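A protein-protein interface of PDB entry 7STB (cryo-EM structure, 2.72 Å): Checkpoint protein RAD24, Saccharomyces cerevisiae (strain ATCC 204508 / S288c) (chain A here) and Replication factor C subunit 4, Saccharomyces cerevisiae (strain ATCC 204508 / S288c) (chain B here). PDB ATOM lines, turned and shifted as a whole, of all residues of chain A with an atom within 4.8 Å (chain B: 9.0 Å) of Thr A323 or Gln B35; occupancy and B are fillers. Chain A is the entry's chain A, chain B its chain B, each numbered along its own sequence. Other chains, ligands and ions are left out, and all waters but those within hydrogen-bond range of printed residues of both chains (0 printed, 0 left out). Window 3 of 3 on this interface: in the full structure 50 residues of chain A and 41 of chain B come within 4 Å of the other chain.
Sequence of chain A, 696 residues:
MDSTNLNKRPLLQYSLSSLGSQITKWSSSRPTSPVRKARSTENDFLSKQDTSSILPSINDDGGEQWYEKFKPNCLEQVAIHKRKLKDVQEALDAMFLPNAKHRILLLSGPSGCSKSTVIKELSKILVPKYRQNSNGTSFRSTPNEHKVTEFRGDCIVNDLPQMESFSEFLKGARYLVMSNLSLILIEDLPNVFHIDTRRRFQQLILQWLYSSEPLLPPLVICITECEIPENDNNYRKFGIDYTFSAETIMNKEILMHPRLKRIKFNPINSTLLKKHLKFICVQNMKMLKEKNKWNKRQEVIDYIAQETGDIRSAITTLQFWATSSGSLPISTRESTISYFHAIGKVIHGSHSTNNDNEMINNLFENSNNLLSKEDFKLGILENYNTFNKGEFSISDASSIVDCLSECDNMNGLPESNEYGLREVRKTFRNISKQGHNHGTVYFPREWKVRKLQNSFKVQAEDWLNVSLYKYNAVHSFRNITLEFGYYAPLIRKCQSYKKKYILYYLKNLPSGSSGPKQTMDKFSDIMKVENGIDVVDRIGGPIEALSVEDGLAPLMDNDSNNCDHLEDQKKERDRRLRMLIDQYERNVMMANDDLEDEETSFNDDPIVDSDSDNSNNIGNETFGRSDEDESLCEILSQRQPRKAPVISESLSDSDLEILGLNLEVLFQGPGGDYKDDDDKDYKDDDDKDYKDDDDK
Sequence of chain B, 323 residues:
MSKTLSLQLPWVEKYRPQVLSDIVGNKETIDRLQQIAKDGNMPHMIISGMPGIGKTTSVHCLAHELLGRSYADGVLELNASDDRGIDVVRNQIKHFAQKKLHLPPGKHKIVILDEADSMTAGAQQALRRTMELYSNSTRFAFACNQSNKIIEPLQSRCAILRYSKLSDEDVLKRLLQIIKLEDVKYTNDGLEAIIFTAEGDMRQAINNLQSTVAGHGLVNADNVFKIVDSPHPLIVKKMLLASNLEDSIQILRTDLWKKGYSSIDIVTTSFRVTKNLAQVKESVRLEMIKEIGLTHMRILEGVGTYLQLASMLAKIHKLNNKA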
ATOM      1  N   MET A 287      24.927 -19.568  24.113  1.00  0.00           N
ATOM      2  CA  MET A 287      24.362 -18.336  23.573  1.00  0.00           C
ATOM      3  C   MET A 287      24.821 -18.098  22.139  1.00  0.00           C
ATOM      4  O   MET A 287      24.036 -17.641  21.300  1.00  0.00           O
ATOM      5  CB  MET A 287      24.731 -17.152  24.472  1.00  0.00           C
ATOM      6  CG  MET A 287      26.224 -16.879  24.610  1.00  0.00           C
ATOM      7  SD  MET A 287      26.935 -15.995  23.208  1.00  0.00           S
ATOM      8  CE  MET A 287      26.218 -14.368  23.427  1.00  0.00           C
ATOM      9  N   LYS A 291      22.086 -17.773  19.153  1.00  0.00           N
ATOM     10  CA  LYS A 291      21.973 -16.544  18.381  1.00  0.00           C
ATOM     11  C   LYS A 291      22.462 -16.706  16.946  1.00  0.00           C
ATOM     12  O   LYS A 291      22.347 -15.765  16.155  1.00  0.00           O
ATOM     13  CB  LYS A 291      22.748 -15.425  19.089  1.00  0.00           C
ATOM     14  CG  LYS A 291      22.611 -14.043  18.469  1.00  0.00           C
ATOM     15  CD  LYS A 291      23.465 -13.030  19.212  1.00  0.00           C
ATOM     16  CE  LYS A 291      22.859 -12.684  20.562  1.00  0.00           C
ATOM     17  NZ  LYS A 291      23.614 -11.610  21.258  1.00  0.00           N
ATOM     18  N   GLN A 319      33.146  -9.766  23.599  1.00  0.00           N
ATOM     19  CA  GLN A 319      31.919  -9.782  24.389  1.00  0.00           C
ATOM     20  C   GLN A 319      30.884  -8.827  23.810  1.00  0.00           C
ATOM     21  O   GLN A 319      29.695  -9.159  23.736  1.00  0.00           O
ATOM     22  CB  GLN A 319      32.220  -9.419  25.842  1.00  0.00           C
ATOM     23  CG  GLN A 319      31.012  -9.532  26.762  1.00  0.00           C
ATOM     24  CD  GLN A 319      31.318  -9.113  28.184  1.00  0.00           C
ATOM     25  OE1 GLN A 319      32.416  -8.646  28.483  1.00  0.00           O
ATOM     26  NE2 GLN A 319      30.344  -9.277  29.070  1.00  0.00           N
ATOM     27  N   PHE A 320      31.315  -7.634  23.399  1.00  0.00           N
ATOM     28  CA  PHE A 320      30.380  -6.667  22.837  1.00  0.00           C
ATOM     29  C   PHE A 320      29.740  -7.204  21.564  1.00  0.00           C
ATOM     30  O   PHE A 320      28.532  -7.050  21.353  1.00  0.00           O
ATOM     31  CB  PHE A 320      31.100  -5.345  22.568  1.00  0.00           C
ATOM     32  CG  PHE A 320      30.177  -4.193  22.300  1.00  0.00           C
ATOM     33  CD1 PHE A 320      29.359  -3.694  23.301  1.00  0.00           C
ATOM     34  CD2 PHE A 320      30.140  -3.594  21.053  1.00  0.00           C
ATOM     35  CE1 PHE A 320      28.514  -2.631  23.059  1.00  0.00           C
ATOM     36  CE2 PHE A 320      29.296  -2.530  20.806  1.00  0.00           C
ATOM     37  CZ  PHE A 320      28.482  -2.048  21.810  1.00  0.00           C
ATOM     38  N   TRP A 321      30.537  -7.839  20.701  1.00  0.00           N
ATOM     39  CA  TRP A 321      29.989  -8.423  19.481  1.00  0.00           C
ATOM     40  C   TRP A 321      29.028  -9.562  19.795  1.00  0.00           C
ATOM     41  O   TRP A 321      27.943  -9.645  19.206  1.00  0.00           O
ATOM     42  CB  TRP A 321      31.124  -8.914  18.583  1.00  0.00           C
ATOM     43  CG  TRP A 321      30.723 -10.015  17.643  1.00  0.00           C
ATOM     44  CD1 TRP A 321      30.091  -9.878  16.443  1.00  0.00           C
ATOM     45  CD2 TRP A 321      30.932 -11.421  17.827  1.00  0.00           C
ATOM     46  NE1 TRP A 321      29.891 -11.110  15.869  1.00  0.00           N
ATOM     47  CE2 TRP A 321      30.398 -12.074  16.700  1.00  0.00           C
ATOM     48  CE3 TRP A 321      31.516 -12.191  18.837  1.00  0.00           C
ATOM     49  CZ2 TRP A 321      30.432 -13.458  16.552  1.00  0.00           C
ATOM     50  CZ3 TRP A 321      31.548 -13.566  18.689  1.00  0.00           C
ATOM     51  CH2 TRP A 321      31.010 -14.184  17.556  1.00  0.00           C
ATOM     52  N   ALA A 322      29.404 -10.449  20.719  1.00  0.00           N
ATOM     53  CA  ALA A 322      28.563 -11.601  21.024  1.00  0.00           C
ATOM     54  C   ALA A 322      27.235 -11.176  21.640  1.00  0.00           C
ATOM     55  O   ALA A 322      26.184 -11.734  21.306  1.00  0.00           O
ATOM     56  CB  ALA A 322      29.304 -12.557  21.957  1.00  0.00           C
ATOM     57  N   THR A 323      27.262 -10.195  22.545  1.00  0.00           N
ATOM     58  CA  THR A 323      26.040  -9.798  23.238  1.00  0.00           C
ATOM     59  C   THR A 323      25.071  -9.079  22.309  1.00  0.00           C
ATOM     60  O   THR A 323      23.860  -9.088  22.556  1.00  0.00           O
ATOM     61  CB  THR A 323      26.380  -8.910  24.434  1.00  0.00           C
ATOM     62  OG1 THR A 323      27.401  -9.532  25.223  1.00  0.00           O
ATOM     63  CG2 THR A 323      25.148  -8.681  25.299  1.00  0.00           C
ATOM     64  N   SER A 324      25.573  -8.454  21.247  1.00  0.00           N
ATOM     65  CA  SER A 324      24.706  -7.712  20.340  1.00  0.00           C
ATOM     66  C   SER A 324      23.780  -8.666  19.595  1.00  0.00           C
ATOM     67  O   SER A 324      24.229  -9.655  19.008  1.00  0.00           O
ATOM     68  CB  SER A 324      25.544  -6.906  19.350  1.00  0.00           C
ATOM     69  OG  SER A 324      25.885  -7.685  18.218  1.00  0.00           O
ATOM     70  N   SER A 325      22.481  -8.364  19.622  1.00  0.00           N
ATOM     71  CA  SER A 325      21.502  -9.215  18.955  1.00  0.00           C
ATOM     72  C   SER A 325      21.513  -8.998  17.447  1.00  0.00           C
ATOM     73  O   SER A 325      21.319  -9.947  16.679  1.00  0.00           O
ATOM     74  CB  SER A 325      20.107  -8.949  19.520  1.00  0.00           C
ATOM     75  OG  SER A 325      19.681  -7.630  19.226  1.00  0.00           O
ATOM     76  N   GLY A 326      21.737  -7.763  17.009  1.00  0.00           N
ATOM     77  CA  GLY A 326      21.780  -7.457  15.594  1.00  0.00           C
ATOM     78  C   GLY A 326      23.152  -7.693  15.001  1.00  0.00           C
ATOM     79  O   GLY A 326      23.741  -8.762  15.191  1.00  0.00           O
ATOM     80  N   LEU B  20      15.297   6.929  23.792  1.00  0.00           N
ATOM     81  CA  LEU B  20      16.222   6.677  22.694  1.00  0.00           C
ATOM     82  C   LEU B  20      15.504   6.490  21.366  1.00  0.00           C
ATOM     83  O   LEU B  20      16.100   6.736  20.311  1.00  0.00           O
ATOM     84  CB  LEU B  20      17.070   5.443  22.999  1.00  0.00           C
ATOM     85  CG  LEU B  20      18.165   5.613  24.053  1.00  0.00           C
ATOM     86  CD1 LEU B  20      18.545   4.270  24.650  1.00  0.00           C
ATOM     87  CD2 LEU B  20      19.384   6.303  23.462  1.00  0.00           C
ATOM     88  N   LYS B  27      21.101   4.609  13.196  1.00  0.00           N
ATOM     89  CA  LYS B  27      20.092   3.664  13.665  1.00  0.00           C
ATOM     90  C   LYS B  27      20.721   2.428  14.296  1.00  0.00           C
ATOM     91  O   LYS B  27      20.187   1.879  15.266  1.00  0.00           O
ATOM     92  CB  LYS B  27      19.179   3.266  12.503  1.00  0.00           C
ATOM     93  CG  LYS B  27      18.059   2.308  12.885  1.00  0.00           C
ATOM     94  CD  LYS B  27      17.211   1.939  11.677  1.00  0.00           C
ATOM     95  CE  LYS B  27      16.092   0.983  12.055  1.00  0.00           C
ATOM     96  NZ  LYS B  27      16.610  -0.352  12.465  1.00  0.00           N
ATOM     97  N   GLU B  28      21.854   1.971  13.762  1.00  0.00           N
ATOM     98  CA  GLU B  28      22.472   0.753  14.277  1.00  0.00           C
ATOM     99  C   GLU B  28      22.938   0.938  15.718  1.00  0.00           C
ATOM    100  O   GLU B  28      22.647   0.109  16.590  1.00  0.00           O
ATOM    101  CB  GLU B  28      23.641   0.345  13.377  1.00  0.00           C
ATOM    102  CG  GLU B  28      24.333  -0.941  13.795  1.00  0.00           C
ATOM    103  CD  GLU B  28      23.429  -2.151  13.680  1.00  0.00           C
ATOM    104  OE1 GLU B  28      22.488  -2.116  12.860  1.00  0.00           O
ATOM    105  OE2 GLU B  28      23.658  -3.139  14.409  1.00  0.00           O
ATOM    106  N   THR B  29      23.660   2.027  15.990  1.00  0.00           N
ATOM    107  CA  THR B  29      24.157   2.258  17.342  1.00  0.00           C
ATOM    108  C   THR B  29      23.014   2.523  18.313  1.00  0.00           C
ATOM    109  O   THR B  29      23.067   2.100  19.471  1.00  0.00           O
ATOM    110  CB  THR B  29      25.145   3.424  17.351  1.00  0.00           C
ATOM    111  OG1 THR B  29      24.549   4.563  16.724  1.00  0.00           O
ATOM    112  CG2 THR B  29      26.419   3.050  16.610  1.00  0.00           C
ATOM    113  N   ILE B  30      21.971   3.226  17.865  1.00  0.00           N
ATOM    114  CA  ILE B  30      20.832   3.484  18.741  1.00  0.00           C
ATOM    115  C   ILE B  30      20.105   2.185  19.068  1.00  0.00           C
ATOM    116  O   ILE B  30      19.653   1.981  20.200  1.00  0.00           O
ATOM    117  CB  ILE B  30      19.885   4.523  18.111  1.00  0.00           C
ATOM    118  CG1 ILE B  30      20.657   5.777  17.684  1.00  0.00           C
ATOM    119  CG2 ILE B  30      18.774   4.887  19.083  1.00  0.00           C
ATOM    120  CD1 ILE B  30      21.244   6.569  18.836  1.00  0.00           C
ATOM    121  N   ASP B  31      19.976   1.288  18.088  1.00  0.00           N
ATOM    122  CA  ASP B  31      19.388  -0.019  18.363  1.00  0.00           C
ATOM    123  C   ASP B  31      20.248  -0.810  19.341  1.00  0.00           C
ATOM    124  O   ASP B  31      19.726  -1.498  20.227  1.00  0.00           O
ATOM    125  CB  ASP B  31      19.204  -0.796  17.060  1.00  0.00           C
ATOM    126  CG  ASP B  31      18.135  -0.195  16.169  1.00  0.00           C
ATOM    127  OD1 ASP B  31      17.188   0.420  16.704  1.00  0.00           O
ATOM    128  OD2 ASP B  31      18.239  -0.337  14.932  1.00  0.00           O
ATOM    129  N   ARG B  32      21.571  -0.731  19.190  1.00  0.00           N
ATOM    130  CA  ARG B  32      22.457  -1.393  20.143  1.00  0.00           C
ATOM    131  C   ARG B  32      22.263  -0.832  21.546  1.00  0.00           C
ATOM    132  O   ARG B  32      22.241  -1.584  22.528  1.00  0.00           O
ATOM    133  CB  ARG B  32      23.911  -1.242  19.697  1.00  0.00           C
ATOM    134  CG  ARG B  32      24.913  -2.016  20.545  1.00  0.00           C
ATOM    135  CD  ARG B  32      25.043  -3.456  20.080  1.00  0.00           C
ATOM    136  NE  ARG B  32      25.780  -4.277  21.033  1.00  0.00           N
ATOM    137  CZ  ARG B  32      25.281  -4.734  22.174  1.00  0.00           C
ATOM    138  NH1 ARG B  32      24.037  -4.471  22.540  1.00  0.00           N
ATOM    139  NH2 ARG B  32      26.049  -5.476  22.967  1.00  0.00           N
ATOM    140  N   LEU B  33      22.127   0.489  21.662  1.00  0.00           N
ATOM    141  CA  LEU B  33      21.900   1.103  22.967  1.00  0.00           C
ATOM    142  C   LEU B  33      20.559   0.675  23.551  1.00  0.00           C
ATOM    143  O   LEU B  33      20.442   0.462  24.763  1.00  0.00           O
ATOM    144  CB  LEU B  33      21.976   2.625  22.851  1.00  0.00           C
ATOM    145  CG  LEU B  33      23.340   3.209  22.469  1.00  0.00           C
ATOM    146  CD1 LEU B  33      23.249   4.718  22.325  1.00  0.00           C
ATOM    147  CD2 LEU B  33      24.414   2.832  23.481  1.00  0.00           C
ATOM    148  N   GLN B  34      19.531   0.555  22.708  1.00  0.00           N
ATOM    149  CA  GLN B  34      18.244   0.049  23.175  1.00  0.00           C
ATOM    150  C   GLN B  34      18.364  -1.375  23.699  1.00  0.00           C
ATOM    151  O   GLN B  34      17.793  -1.713  24.743  1.00  0.00           O
ATOM    152  CB  GLN B  34      17.212   0.119  22.050  1.00  0.00           C
ATOM    153  CG  GLN B  34      16.388   1.389  22.055  1.00  0.00           C
ATOM    154  CD  GLN B  34      15.435   1.438  23.234  1.00  0.00           C
ATOM    155  OE1 GLN B  34      15.544   2.311  24.096  1.00  0.00           O
ATOM    156  NE2 GLN B  34      14.478   0.522  23.263  1.00  0.00           N
ATOM    157  N   GLN B  35      19.097  -2.229  22.983  1.00  0.00           N
ATOM    158  CA  GLN B  35      19.296  -3.592  23.462  1.00  0.00           C
ATOM    159  C   GLN B  35      20.064  -3.599  24.778  1.00  0.00           C
ATOM    160  O   GLN B  35      19.772  -4.398  25.674  1.00  0.00           O
ATOM    161  CB  GLN B  35      20.026  -4.425  22.411  1.00  0.00           C
ATOM    162  CG  GLN B  35      20.144  -5.897  22.777  1.00  0.00           C
ATOM    163  CD  GLN B  35      21.227  -6.608  21.998  1.00  0.00           C
ATOM    164  OE1 GLN B  35      21.717  -6.102  20.988  1.00  0.00           O
ATOM    165  NE2 GLN B  35      21.610  -7.792  22.463  1.00  0.00           N
ATOM    166  N   ILE B  36      21.061  -2.721  24.906  1.00  0.00           N
ATOM    167  CA  ILE B  36      21.812  -2.623  26.156  1.00  0.00           C
ATOM    168  C   ILE B  36      20.885  -2.223  27.295  1.00  0.00           C
ATOM    169  O   ILE B  36      20.939  -2.792  28.391  1.00  0.00           O
ATOM    170  CB  ILE B  36      22.978  -1.629  26.001  1.00  0.00           C
ATOM    171  CG1 ILE B  36      24.066  -2.222  25.103  1.00  0.00           C
ATOM    172  CG2 ILE B  36      23.553  -1.266  27.363  1.00  0.00           C
ATOM    173  CD1 ILE B  36      25.038  -1.196  24.560  1.00  0.00           C
ATOM    174  N   ALA B  37      20.023  -1.235  27.054  1.00  0.00           N
ATOM    175  CA  ALA B  37      19.092  -0.793  28.086  1.00  0.00           C
ATOM    176  C   ALA B  37      18.138  -1.913  28.478  1.00  0.00           C
ATOM    177  O   ALA B  37      17.841  -2.098  29.664  1.00  0.00           O
ATOM    178  CB  ALA B  37      18.314   0.430  27.600  1.00  0.00           C
ATOM    179  N   LYS B  38      17.644  -2.668  27.496  1.00  0.00           N
ATOM    180  CA  LYS B  38      16.733  -3.767  27.803  1.00  0.00           C
ATOM    181  C   LYS B  38      17.433  -4.847  28.617  1.00  0.00           C
ATOM    182  O   LYS B  38      16.925  -5.281  29.659  1.00  0.00           O
ATOM    183  CB  LYS B  38      16.166  -4.353  26.511  1.00  0.00           C
ATOM    184  CG  LYS B  38      15.020  -5.328  26.734  1.00  0.00           C
ATOM    185  CD  LYS B  38      14.368  -5.737  25.424  1.00  0.00           C
ATOM    186  CE  LYS B  38      15.193  -6.790  24.702  1.00  0.00           C
ATOM    187  NZ  LYS B  38      14.489  -7.332  23.507  1.00  0.00           N
ATOM    188  N   ASP B  39      18.604  -5.294  28.160  1.00  0.00           N
ATOM    189  CA  ASP B  39      19.341  -6.324  28.886  1.00  0.00           C
ATOM    190  C   ASP B  39      19.846  -5.797  30.223  1.00  0.00           C
ATOM    191  O   ASP B  39      19.758  -6.486  31.246  1.00  0.00           O
ATOM    192  CB  ASP B  39      20.503  -6.832  28.033  1.00  0.00           C
ATOM    193  CG  ASP B  39      20.058  -7.800  26.956  1.00  0.00           C
ATOM    194  OD1 ASP B  39      18.838  -8.042  26.839  1.00  0.00           O
ATOM    195  OD2 ASP B  39      20.927  -8.322  26.227  1.00  0.00           O
ATOM    196  N   GLY B  40      20.380  -4.577  30.234  1.00  0.00           N
ATOM    197  CA  GLY B  40      20.845  -3.943  31.448  1.00  0.00           C
ATOM    198  C   GLY B  40      22.312  -4.152  31.758  1.00  0.00           C
ATOM    199  O   GLY B  40      22.817  -3.542  32.708  1.00  0.00           O
ATOM    200  N   ASN B  41      23.007  -4.991  30.994  1.00  0.00           N
ATOM    201  CA  ASN B  41      24.412  -5.301  31.261  1.00  0.00           C
ATOM    202  C   ASN B  41      25.298  -4.292  30.527  1.00  0.00           C
ATOM    203  O   ASN B  41      26.009  -4.601  29.570  1.00  0.00           O
ATOM    204  CB  ASN B  41      24.720  -6.734  30.848  1.00  0.00           C
ATOM    205  CG  ASN B  41      24.703  -7.697  32.020  1.00  0.00           C
ATOM    206  OD1 ASN B  41      24.684  -7.285  33.179  1.00  0.00           O
ATOM    207  ND2 ASN B  41      24.703  -8.990  31.721  1.00  0.00           N
ATOM    208  N   MET B  42      25.237  -3.055  31.005  1.00  0.00           N
ATOM    209  CA  MET B  42      25.952  -1.958  30.365  1.00  0.00           C
ATOM    210  C   MET B  42      27.435  -2.035  30.706  1.00  0.00           C
ATOM    211  O   MET B  42      27.788  -2.037  31.890  1.00  0.00           O
ATOM    212  CB  MET B  42      25.377  -0.623  30.821  1.00  0.00           C
ATOM    213  CG  MET B  42      25.968   0.592  30.126  1.00  0.00           C
ATOM    214  SD  MET B  42      25.771   2.089  31.109  1.00  0.00           S
ATOM    215  CE  MET B  42      26.673   3.273  30.117  1.00  0.00           C
ATOM    216  N   PRO B  43      28.334  -2.107  29.713  1.00  0.00           N
ATOM    217  CA  PRO B  43      29.769  -2.077  30.017  1.00  0.00           C
ATOM    218  C   PRO B  43      30.329  -0.664  30.007  1.00  0.00           C
ATOM    219  O   PRO B  43      29.603   0.290  29.714  1.00  0.00           O
ATOM    220  CB  PRO B  43      30.371  -2.926  28.894  1.00  0.00           C
ATOM    221  CG  PRO B  43      29.476  -2.647  27.725  1.00  0.00           C
ATOM    222  CD  PRO B  43      28.093  -2.347  28.279  1.00  0.00           C
ATOM    223  N   LEU B  62      19.918   6.734  27.752  1.00  0.00           N
ATOM    224  CA  LEU B  62      20.269   5.382  28.175  1.00  0.00           C
ATOM    225  C   LEU B  62      20.301   5.275  29.692  1.00  0.00           C
ATOM    226  O   LEU B  62      19.780   4.310  30.264  1.00  0.00           O
ATOM    227  CB  LEU B  62      21.619   4.981  27.580  1.00  0.00           C
ATOM    228  CG  LEU B  62      22.092   3.567  27.920  1.00  0.00           C
ATOM    229  CD1 LEU B  62      22.694   2.899  26.701  1.00  0.00           C
ATOM    230  CD2 LEU B  62      23.103   3.600  29.056  1.00  0.00           C
ATOM    231  N   GLU B  65      16.655   5.340  31.001  1.00  0.00           N
ATOM    232  CA  GLU B  65      15.966   4.077  30.766  1.00  0.00           C
ATOM    233  C   GLU B  65      16.503   2.981  31.677  1.00  0.00           C
ATOM    234  O   GLU B  65      15.739   2.140  32.164  1.00  0.00           O
ATOM    235  CB  GLU B  65      16.107   3.670  29.300  1.00  0.00           C
ATOM    236  CG  GLU B  65      14.956   2.825  28.782  1.00  0.00           C
ATOM    237  CD  GLU B  65      14.865   2.828  27.271  1.00  0.00           C
ATOM    238  OE1 GLU B  65      14.481   1.788  26.694  1.00  0.00           O
ATOM    239  OE2 GLU B  65      15.176   3.869  26.655  1.00  0.00           O
ATOM    240  N   LEU B  66      17.814   2.972  31.917  1.00  0.00           N
ATOM    241  CA  LEU B  66      18.404   1.935  32.754  1.00  0.00           C
ATOM    242  C   LEU B  66      17.959   2.075  34.204  1.00  0.00           C
ATOM    243  O   LEU B  66      17.615   1.081  34.853  1.00  0.00           O
ATOM    244  CB  LEU B  66      19.929   1.990  32.653  1.00  0.00           C
ATOM    245  CG  LEU B  66      20.563   1.182  31.518  1.00  0.00           C
ATOM    246  CD1 LEU B  66      22.044   1.492  31.410  1.00  0.00           C
ATOM    247  CD2 LEU B  66      20.347  -0.308  31.722  1.00  0.00           C
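The backbone NH (N) of Ser A325 is in hydrogen-bond range of the side-chain amide oxygen (OE1) of Gln B35.
The side-chain amide nitrogen (NE2) of Gln B35 sits at hydrogen-bond distance from the backbone carbonyl oxygen (O) of Thr A323 (2.6 Å).
NH2 of Arg B32 lies within hydrogen-bond range of O of Phe A320 (3.4 Å).
The backbone NH of Ser A324 lies close to the guanidinium group of Arg B32 (3.5 Å).
The backbone carbonyl oxygen (O) of Ser A324 is in hydrogen-bond range of the side-chain amino group (NZ) of Lys A291 (3.0 Å).
The backbone carbonyl oxygen (O) of Gln A319 sits at hydrogen-bond distance from the side-chain hydroxyl (OG1) of Thr A323 (2.8 Å).
The guanidinium group (NH1) of Arg B32 sits at hydrogen-bond distance from the side-chain amide oxygen (OE1) of Gln B35 (3.2 Å).
The backbone carbonyl oxygen of Thr A323 is in hydrogen-bond range of the side-chain amino group of Lys A291 (2.8 Å).
The side-chain hydroxyl of Ser A324 sits at hydrogen-bond distance from the backbone carbonyl oxygen of Trp A321 (3.0 Å).
Among the printed residues, merely in contact across the chains: Ser A324 with Gln B35 (3.5 Å) and Thr A323 with Arg B32 (3.7 Å).
Of the printed residues of chain B, Phe A320 touches Arg B32.
No residue of chain B comes within 4 Å of Ala A322.
Ser A324 touches just these residues of chain B: Arg B32 (3.1 Å) and Gln B35 (3.5 Å).
Printed residues of chain B within 4 Å of Ser A325: Gln B35 (2.8 Å).
Of the printed residues of chain A, Arg B32 touches Phe A320 (3.4 Å), Thr A323 (3.7 Å) and Ser A324 (3.1 Å).
Of chain A, only Thr A323, Ser A324 and Ser A325 come within 4 Å of Gln B35.
The nearest residue of chain A that does not touch Gln B35 is Gly A326 (4.3 Å).
Of the 10 printed residues of chain A, 4 touch a printed residue of chain B.
Hydrophobic or aromatic side chains of chain A that line the printed part of chain B: Phe A320.
Among the printed residues, no Asp or Glu carboxylate lies within 4 Å of a Lys or Arg side-chain nitrogen of the other chain.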
